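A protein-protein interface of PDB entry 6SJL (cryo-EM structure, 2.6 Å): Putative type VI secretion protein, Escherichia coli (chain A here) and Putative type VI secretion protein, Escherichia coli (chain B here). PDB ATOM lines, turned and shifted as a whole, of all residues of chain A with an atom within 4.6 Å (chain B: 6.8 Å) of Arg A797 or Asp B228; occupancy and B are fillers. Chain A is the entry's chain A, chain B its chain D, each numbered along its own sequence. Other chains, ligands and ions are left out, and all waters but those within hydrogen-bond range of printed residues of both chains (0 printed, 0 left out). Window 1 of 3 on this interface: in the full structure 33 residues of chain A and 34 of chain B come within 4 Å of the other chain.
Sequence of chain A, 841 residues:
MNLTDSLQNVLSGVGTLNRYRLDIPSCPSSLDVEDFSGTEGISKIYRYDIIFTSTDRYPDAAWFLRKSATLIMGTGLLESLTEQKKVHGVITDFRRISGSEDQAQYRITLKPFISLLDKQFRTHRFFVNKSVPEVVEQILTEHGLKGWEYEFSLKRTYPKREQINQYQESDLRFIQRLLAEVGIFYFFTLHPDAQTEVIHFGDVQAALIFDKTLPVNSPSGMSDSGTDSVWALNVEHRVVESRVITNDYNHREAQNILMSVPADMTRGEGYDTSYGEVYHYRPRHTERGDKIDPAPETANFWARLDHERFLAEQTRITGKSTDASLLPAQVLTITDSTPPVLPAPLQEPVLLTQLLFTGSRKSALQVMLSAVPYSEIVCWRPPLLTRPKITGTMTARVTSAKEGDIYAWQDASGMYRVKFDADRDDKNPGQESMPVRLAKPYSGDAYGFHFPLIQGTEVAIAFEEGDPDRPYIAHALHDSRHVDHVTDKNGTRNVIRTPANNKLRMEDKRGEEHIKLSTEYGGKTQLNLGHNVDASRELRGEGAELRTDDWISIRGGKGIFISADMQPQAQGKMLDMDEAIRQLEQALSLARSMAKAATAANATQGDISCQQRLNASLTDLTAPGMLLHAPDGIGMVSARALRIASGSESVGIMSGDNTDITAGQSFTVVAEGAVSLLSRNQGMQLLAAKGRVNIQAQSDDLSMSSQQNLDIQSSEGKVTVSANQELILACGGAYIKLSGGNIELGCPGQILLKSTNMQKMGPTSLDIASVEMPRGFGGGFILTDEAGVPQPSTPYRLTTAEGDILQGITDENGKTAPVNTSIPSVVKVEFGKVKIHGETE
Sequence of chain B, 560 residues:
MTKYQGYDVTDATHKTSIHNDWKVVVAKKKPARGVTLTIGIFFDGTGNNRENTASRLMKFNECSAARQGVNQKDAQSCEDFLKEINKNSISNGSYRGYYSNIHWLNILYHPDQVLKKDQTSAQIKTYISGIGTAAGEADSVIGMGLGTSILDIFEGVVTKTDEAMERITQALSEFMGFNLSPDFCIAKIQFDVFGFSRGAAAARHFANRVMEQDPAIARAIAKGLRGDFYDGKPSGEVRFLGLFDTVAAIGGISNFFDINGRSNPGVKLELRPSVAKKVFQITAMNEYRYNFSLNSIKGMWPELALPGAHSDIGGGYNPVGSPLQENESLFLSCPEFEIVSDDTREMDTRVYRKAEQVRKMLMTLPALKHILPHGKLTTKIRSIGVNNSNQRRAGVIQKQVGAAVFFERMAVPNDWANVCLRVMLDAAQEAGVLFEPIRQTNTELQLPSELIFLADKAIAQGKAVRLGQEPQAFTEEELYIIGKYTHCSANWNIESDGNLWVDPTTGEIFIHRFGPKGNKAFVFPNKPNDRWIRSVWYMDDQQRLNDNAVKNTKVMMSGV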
ATOM      1  N   TYR A 796       4.607  -2.799  22.056  1.00  0.00           N
ATOM      2  CA  TYR A 796       3.527  -3.693  22.444  1.00  0.00           C
ATOM      3  C   TYR A 796       3.908  -4.372  23.748  1.00  0.00           C
ATOM      4  O   TYR A 796       5.065  -4.348  24.170  1.00  0.00           O
ATOM      5  CB  TYR A 796       3.236  -4.731  21.355  1.00  0.00           C
ATOM      6  CG  TYR A 796       4.317  -5.778  21.174  1.00  0.00           C
ATOM      7  CD1 TYR A 796       5.255  -5.668  20.160  1.00  0.00           C
ATOM      8  CD2 TYR A 796       4.391  -6.883  22.013  1.00  0.00           C
ATOM      9  CE1 TYR A 796       6.241  -6.620  19.997  1.00  0.00           C
ATOM     10  CE2 TYR A 796       5.373  -7.831  21.861  1.00  0.00           C
ATOM     11  CZ  TYR A 796       6.293  -7.697  20.849  1.00  0.00           C
ATOM     12  OH  TYR A 796       7.271  -8.647  20.688  1.00  0.00           O
ATOM     13  N   ARG A 797       2.926  -5.010  24.375  1.00  0.00           N
ATOM     14  CA  ARG A 797       3.196  -5.771  25.590  1.00  0.00           C
ATOM     15  C   ARG A 797       2.277  -6.980  25.619  1.00  0.00           C
ATOM     16  O   ARG A 797       1.053  -6.831  25.611  1.00  0.00           O
ATOM     17  CB  ARG A 797       3.020  -4.913  26.838  1.00  0.00           C
ATOM     18  CG  ARG A 797       3.400  -5.619  28.131  1.00  0.00           C
ATOM     19  CD  ARG A 797       3.580  -4.628  29.271  1.00  0.00           C
ATOM     20  NE  ARG A 797       2.341  -3.946  29.609  1.00  0.00           N
ATOM     21  CZ  ARG A 797       2.126  -2.654  29.402  1.00  0.00           C
ATOM     22  NH1 ARG A 797       3.065  -1.907  28.852  1.00  0.00           N
ATOM     23  NH2 ARG A 797       0.967  -2.113  29.736  1.00  0.00           N
ATOM     24  N   LEU A 798       2.875  -8.164  25.647  1.00  0.00           N
ATOM     25  CA  LEU A 798       2.155  -9.428  25.712  1.00  0.00           C
ATOM     26  C   LEU A 798       2.027  -9.890  27.154  1.00  0.00           C
ATOM     27  O   LEU A 798       2.973  -9.772  27.936  1.00  0.00           O
ATOM     28  CB  LEU A 798       2.869 -10.503  24.899  1.00  0.00           C
ATOM     29  CG  LEU A 798       2.388 -10.740  23.478  1.00  0.00           C
ATOM     30  CD1 LEU A 798       2.250  -9.426  22.757  1.00  0.00           C
ATOM     31  CD2 LEU A 798       3.379 -11.643  22.779  1.00  0.00           C
ATOM     32  N   THR A 799       0.858 -10.421  27.496  1.00  0.00           N
ATOM     33  CA  THR A 799       0.617 -11.028  28.799  1.00  0.00           C
ATOM     34  C   THR A 799      -0.168 -12.320  28.617  1.00  0.00           C
ATOM     35  O   THR A 799      -1.241 -12.320  28.005  1.00  0.00           O
ATOM     36  CB  THR A 799      -0.117 -10.056  29.733  1.00  0.00           C
ATOM     37  OG1 THR A 799      -0.447 -10.715  30.962  1.00  0.00           O
ATOM     38  CG2 THR A 799      -1.359  -9.481  29.085  1.00  0.00           C
ATOM     39  N   ILE A 805       4.882 -11.803  31.376  1.00  0.00           N
ATOM     40  CA  ILE A 805       4.847 -10.618  30.530  1.00  0.00           C
ATOM     41  C   ILE A 805       6.055 -10.635  29.610  1.00  0.00           C
ATOM     42  O   ILE A 805       7.162 -10.984  30.032  1.00  0.00           O
ATOM     43  CB  ILE A 805       4.829  -9.318  31.359  1.00  0.00           C
ATOM     44  CG1 ILE A 805       3.860  -9.430  32.541  1.00  0.00           C
ATOM     45  CG2 ILE A 805       4.464  -8.142  30.478  1.00  0.00           C
ATOM     46  CD1 ILE A 805       2.431  -9.687  32.153  1.00  0.00           C
ATOM     47  N   LEU A 806       5.842 -10.252  28.354  1.00  0.00           N
ATOM     48  CA  LEU A 806       6.929 -10.089  27.383  1.00  0.00           C
ATOM     49  C   LEU A 806       6.585  -8.909  26.473  1.00  0.00           C
ATOM     50  O   LEU A 806       5.851  -9.044  25.491  1.00  0.00           O
ATOM     51  CB  LEU A 806       7.181 -11.379  26.606  1.00  0.00           C
ATOM     52  CG  LEU A 806       6.120 -12.004  25.695  1.00  0.00           C
ATOM     53  CD1 LEU A 806       6.765 -12.906  24.663  1.00  0.00           C
ATOM     54  CD2 LEU A 806       5.122 -12.793  26.526  1.00  0.00           C
ATOM     55  N   GLN A 807       7.108  -7.736  26.813  1.00  0.00           N
ATOM     56  CA  GLN A 807       6.817  -6.575  25.992  1.00  0.00           C
ATOM     57  C   GLN A 807       7.857  -6.446  24.885  1.00  0.00           C
ATOM     58  O   GLN A 807       8.894  -7.111  24.882  1.00  0.00           O
ATOM     59  CB  GLN A 807       6.769  -5.301  26.840  1.00  0.00           C
ATOM     60  CG  GLN A 807       8.116  -4.716  27.235  1.00  0.00           C
ATOM     61  CD  GLN A 807       8.590  -3.660  26.249  1.00  0.00           C
ATOM     62  OE1 GLN A 807       7.779  -2.974  25.629  1.00  0.00           O
ATOM     63  NE2 GLN A 807       9.903  -3.519  26.108  1.00  0.00           N
ATOM     64  N   VAL A 827      -2.899 -11.715  25.719  1.00  0.00           N
ATOM     65  CA  VAL A 827      -3.561 -10.427  25.548  1.00  0.00           C
ATOM     66  C   VAL A 827      -2.593  -9.457  24.877  1.00  0.00           C
ATOM     67  O   VAL A 827      -1.379  -9.678  24.851  1.00  0.00           O
ATOM     68  CB  VAL A 827      -4.062  -9.890  26.907  1.00  0.00           C
ATOM     69  CG1 VAL A 827      -4.919  -8.632  26.746  1.00  0.00           C
ATOM     70  CG2 VAL A 827      -4.829 -10.968  27.643  1.00  0.00           C
ATOM     71  N   LYS A 828      -3.138  -8.370  24.333  1.00  0.00           N
ATOM     72  CA  LYS A 828      -2.369  -7.437  23.527  1.00  0.00           C
ATOM     73  C   LYS A 828      -2.639  -6.003  23.968  1.00  0.00           C
ATOM     74  O   LYS A 828      -3.784  -5.649  24.260  1.00  0.00           O
ATOM     75  CB  LYS A 828      -2.742  -7.579  22.049  1.00  0.00           C
ATOM     76  CG  LYS A 828      -1.776  -6.903  21.139  1.00  0.00           C
ATOM     77  CD  LYS A 828      -0.475  -7.657  21.181  1.00  0.00           C
ATOM     78  CE  LYS A 828       0.640  -6.813  20.656  1.00  0.00           C
ATOM     79  NZ  LYS A 828       0.555  -6.597  19.187  1.00  0.00           N
ATOM     80  N   VAL A 829      -1.581  -5.178  24.003  1.00  0.00           N
ATOM     81  CA  VAL A 829      -1.693  -3.728  24.151  1.00  0.00           C
ATOM     82  C   VAL A 829      -0.592  -3.050  23.345  1.00  0.00           C
ATOM     83  O   VAL A 829       0.434  -3.652  23.030  1.00  0.00           O
ATOM     84  CB  VAL A 829      -1.616  -3.267  25.621  1.00  0.00           C
ATOM     85  CG1 VAL A 829      -2.874  -3.642  26.376  1.00  0.00           C
ATOM     86  CG2 VAL A 829      -0.413  -3.885  26.288  1.00  0.00           C
ATOM     87  N   MET B 176       0.999   4.699  36.465  1.00  0.00           N
ATOM     88  CA  MET B 176       0.387   4.019  35.333  1.00  0.00           C
ATOM     89  C   MET B 176      -0.623   2.979  35.797  1.00  0.00           C
ATOM     90  O   MET B 176      -1.568   2.674  35.067  1.00  0.00           O
ATOM     91  CB  MET B 176       1.457   3.390  34.447  1.00  0.00           C
ATOM     92  CG  MET B 176       2.406   4.405  33.859  1.00  0.00           C
ATOM     93  SD  MET B 176       1.582   5.745  32.985  1.00  0.00           S
ATOM     94  CE  MET B 176       1.066   4.928  31.491  1.00  0.00           C
ATOM     95  N   SER B 181      -4.833   1.019  30.624  1.00  0.00           N
ATOM     96  CA  SER B 181      -5.199   1.189  29.224  1.00  0.00           C
ATOM     97  C   SER B 181      -5.216   2.677  28.914  1.00  0.00           C
ATOM     98  O   SER B 181      -6.293   3.264  28.755  1.00  0.00           O
ATOM     99  CB  SER B 181      -6.559   0.561  28.919  1.00  0.00           C
ATOM    100  OG  SER B 181      -7.595   1.324  29.508  1.00  0.00           O
ATOM    101  N   PRO B 182      -4.054   3.320  28.843  1.00  0.00           N
ATOM    102  CA  PRO B 182      -4.017   4.776  28.691  1.00  0.00           C
ATOM    103  C   PRO B 182      -4.687   5.243  27.411  1.00  0.00           C
ATOM    104  O   PRO B 182      -5.057   4.457  26.540  1.00  0.00           O
ATOM    105  CB  PRO B 182      -2.517   5.094  28.669  1.00  0.00           C
ATOM    106  CG  PRO B 182      -1.874   3.942  29.327  1.00  0.00           C
ATOM    107  CD  PRO B 182      -2.709   2.748  28.990  1.00  0.00           C
ATOM    108  N   ILE B 221      12.896   4.885  34.411  1.00  0.00           N
ATOM    109  CA  ILE B 221      11.679   5.345  33.754  1.00  0.00           C
ATOM    110  C   ILE B 221      11.060   4.217  32.948  1.00  0.00           C
ATOM    111  O   ILE B 221       9.844   4.003  32.984  1.00  0.00           O
ATOM    112  CB  ILE B 221      11.965   6.568  32.869  1.00  0.00           C
ATOM    113  CG1 ILE B 221      12.607   7.683  33.679  1.00  0.00           C
ATOM    114  CG2 ILE B 221      10.691   7.067  32.252  1.00  0.00           C
ATOM    115  CD1 ILE B 221      13.134   8.797  32.846  1.00  0.00           C
ATOM    116  N   ALA B 222      11.890   3.463  32.224  1.00  0.00           N
ATOM    117  CA  ALA B 222      11.379   2.366  31.413  1.00  0.00           C
ATOM    118  C   ALA B 222      10.799   1.261  32.279  1.00  0.00           C
ATOM    119  O   ALA B 222       9.731   0.725  31.973  1.00  0.00           O
ATOM    120  CB  ALA B 222      12.486   1.820  30.520  1.00  0.00           C
ATOM    121  N   GLY B 224       9.499   1.632  35.108  1.00  0.00           N
ATOM    122  CA  GLY B 224       8.276   2.133  35.696  1.00  0.00           C
ATOM    123  C   GLY B 224       7.137   2.142  34.710  1.00  0.00           C
ATOM    124  O   GLY B 224       6.028   1.703  35.017  1.00  0.00           O
ATOM    125  N   LEU B 225       7.403   2.657  33.512  1.00  0.00           N
ATOM    126  CA  LEU B 225       6.429   2.610  32.431  1.00  0.00           C
ATOM    127  C   LEU B 225       6.271   1.214  31.849  1.00  0.00           C
ATOM    128  O   LEU B 225       5.379   1.007  31.025  1.00  0.00           O
ATOM    129  CB  LEU B 225       6.835   3.575  31.328  1.00  0.00           C
ATOM    130  CG  LEU B 225       6.931   5.036  31.726  1.00  0.00           C
ATOM    131  CD1 LEU B 225       7.136   5.886  30.496  1.00  0.00           C
ATOM    132  CD2 LEU B 225       5.681   5.438  32.453  1.00  0.00           C
ATOM    133  N   ARG B 226       7.111   0.262  32.254  1.00  0.00           N
ATOM    134  CA  ARG B 226       7.068  -1.112  31.759  1.00  0.00           C
ATOM    135  C   ARG B 226       7.222  -1.152  30.244  1.00  0.00           C
ATOM    136  O   ARG B 226       6.395  -1.708  29.523  1.00  0.00           O
ATOM    137  CB  ARG B 226       5.795  -1.822  32.211  1.00  0.00           C
ATOM    138  CG  ARG B 226       5.782  -2.125  33.684  1.00  0.00           C
ATOM    139  CD  ARG B 226       4.584  -2.952  34.052  1.00  0.00           C
ATOM    140  NE  ARG B 226       3.383  -2.460  33.394  1.00  0.00           N
ATOM    141  CZ  ARG B 226       2.268  -3.166  33.259  1.00  0.00           C
ATOM    142  NH1 ARG B 226       1.221  -2.638  32.645  1.00  0.00           N
ATOM    143  NH2 ARG B 226       2.199  -4.397  33.745  1.00  0.00           N
ATOM    144  N   GLY B 227       8.302  -0.544  29.764  1.00  0.00           N
ATOM    145  CA  GLY B 227       8.631  -0.552  28.361  1.00  0.00           C
ATOM    146  C   GLY B 227       7.878   0.443  27.511  1.00  0.00           C
ATOM    147  O   GLY B 227       8.203   0.582  26.327  1.00  0.00           O
ATOM    148  N   ASP B 228       6.893   1.143  28.064  1.00  0.00           N
ATOM    149  CA  ASP B 228       6.097   2.063  27.266  1.00  0.00           C
ATOM    150  C   ASP B 228       6.968   3.176  26.697  1.00  0.00           C
ATOM    151  O   ASP B 228       8.149   3.309  27.020  1.00  0.00           O
ATOM    152  CB  ASP B 228       4.964   2.654  28.092  1.00  0.00           C
ATOM    153  CG  ASP B 228       3.964   1.612  28.523  1.00  0.00           C
ATOM    154  OD1 ASP B 228       4.038   0.481  28.014  1.00  0.00           O
ATOM    155  OD2 ASP B 228       3.107   1.921  29.375  1.00  0.00           O
ATOM    156  N   PHE B 229       6.381   3.965  25.815  1.00  0.00           N
ATOM    157  CA  PHE B 229       7.125   5.008  25.131  1.00  0.00           C
ATOM    158  C   PHE B 229       6.989   6.333  25.873  1.00  0.00           C
ATOM    159  O   PHE B 229       5.938   6.635  26.445  1.00  0.00           O
ATOM    160  CB  PHE B 229       6.633   5.139  23.686  1.00  0.00           C
ATOM    161  CG  PHE B 229       7.232   6.288  22.938  1.00  0.00           C
ATOM    162  CD1 PHE B 229       6.477   7.394  22.625  1.00  0.00           C
ATOM    163  CD2 PHE B 229       8.556   6.260  22.549  1.00  0.00           C
ATOM    164  CE1 PHE B 229       7.026   8.448  21.940  1.00  0.00           C
ATOM    165  CE2 PHE B 229       9.108   7.317  21.860  1.00  0.00           C
ATOM    166  CZ  PHE B 229       8.344   8.410  21.559  1.00  0.00           C
ATOM    167  N   TYR B 230       8.069   7.106  25.889  1.00  0.00           N
ATOM    168  CA  TYR B 230       8.017   8.495  26.309  1.00  0.00           C
ATOM    169  C   TYR B 230       8.939   9.292  25.405  1.00  0.00           C
ATOM    170  O   TYR B 230      10.068   8.875  25.147  1.00  0.00           O
ATOM    171  CB  TYR B 230       8.407   8.673  27.787  1.00  0.00           C
ATOM    172  CG  TYR B 230       9.777   8.164  28.175  1.00  0.00           C
ATOM    173  CD1 TYR B 230       9.971   6.843  28.530  1.00  0.00           C
ATOM    174  CD2 TYR B 230      10.863   9.012  28.209  1.00  0.00           C
ATOM    175  CE1 TYR B 230      11.206   6.382  28.881  1.00  0.00           C
ATOM    176  CE2 TYR B 230      12.098   8.559  28.561  1.00  0.00           C
ATOM    177  CZ  TYR B 230      12.267   7.244  28.900  1.00  0.00           C
ATOM    178  OH  TYR B 230      13.509   6.787  29.256  1.00  0.00           O
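Among the printed residues, pairs that only touch across the chains: Gln A807 with Gly B227 (3.6 Å).
N of Arg A797 sits at hydrogen-bond distance from O of Val A829 (3.1 Å). O of Ala B222 lies within hydrogen-bond range of N of Gly B227 (2.9 Å). The backbone carbonyl oxygen (O) of Tyr A796 sits close to the side-chain amide oxygen (OE1) of Gln A807, at 3.4 Å.
Of the 10 printed residues of chain A, 2 touch a printed residue of chain B. Printed residues of chain B that touch a printed residue of chain A: Arg B226, Gly B227 and Asp B228. Among the printed residues, 3 pairs touch across the chains.
OD1 of Asp B228 is in salt-bridge range of NH1 of Arg A797, 2.7 Å away. The guanidinium group (NH1) of Arg A797 sits at hydrogen-bond distance from the backbone carbonyl oxygen (O) of Arg B226.
Arg A797 touches just these residues of chain B: Arg B226 (3.0 Å) and Asp B228 (2.7 Å). Of chain A, only Arg A797 comes within 4 Å of Asp B228. Of the printed residues of chain A, Gly B227 touches Gln A807. Printed residues of chain A within 4 Å of Arg B226: Arg A797 (3.0 Å). Val A827 touches none of the printed residues of chain B. The nearest printed residue of chain A that does not touch Asp B228 is Gln A807 (4.9 Å).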
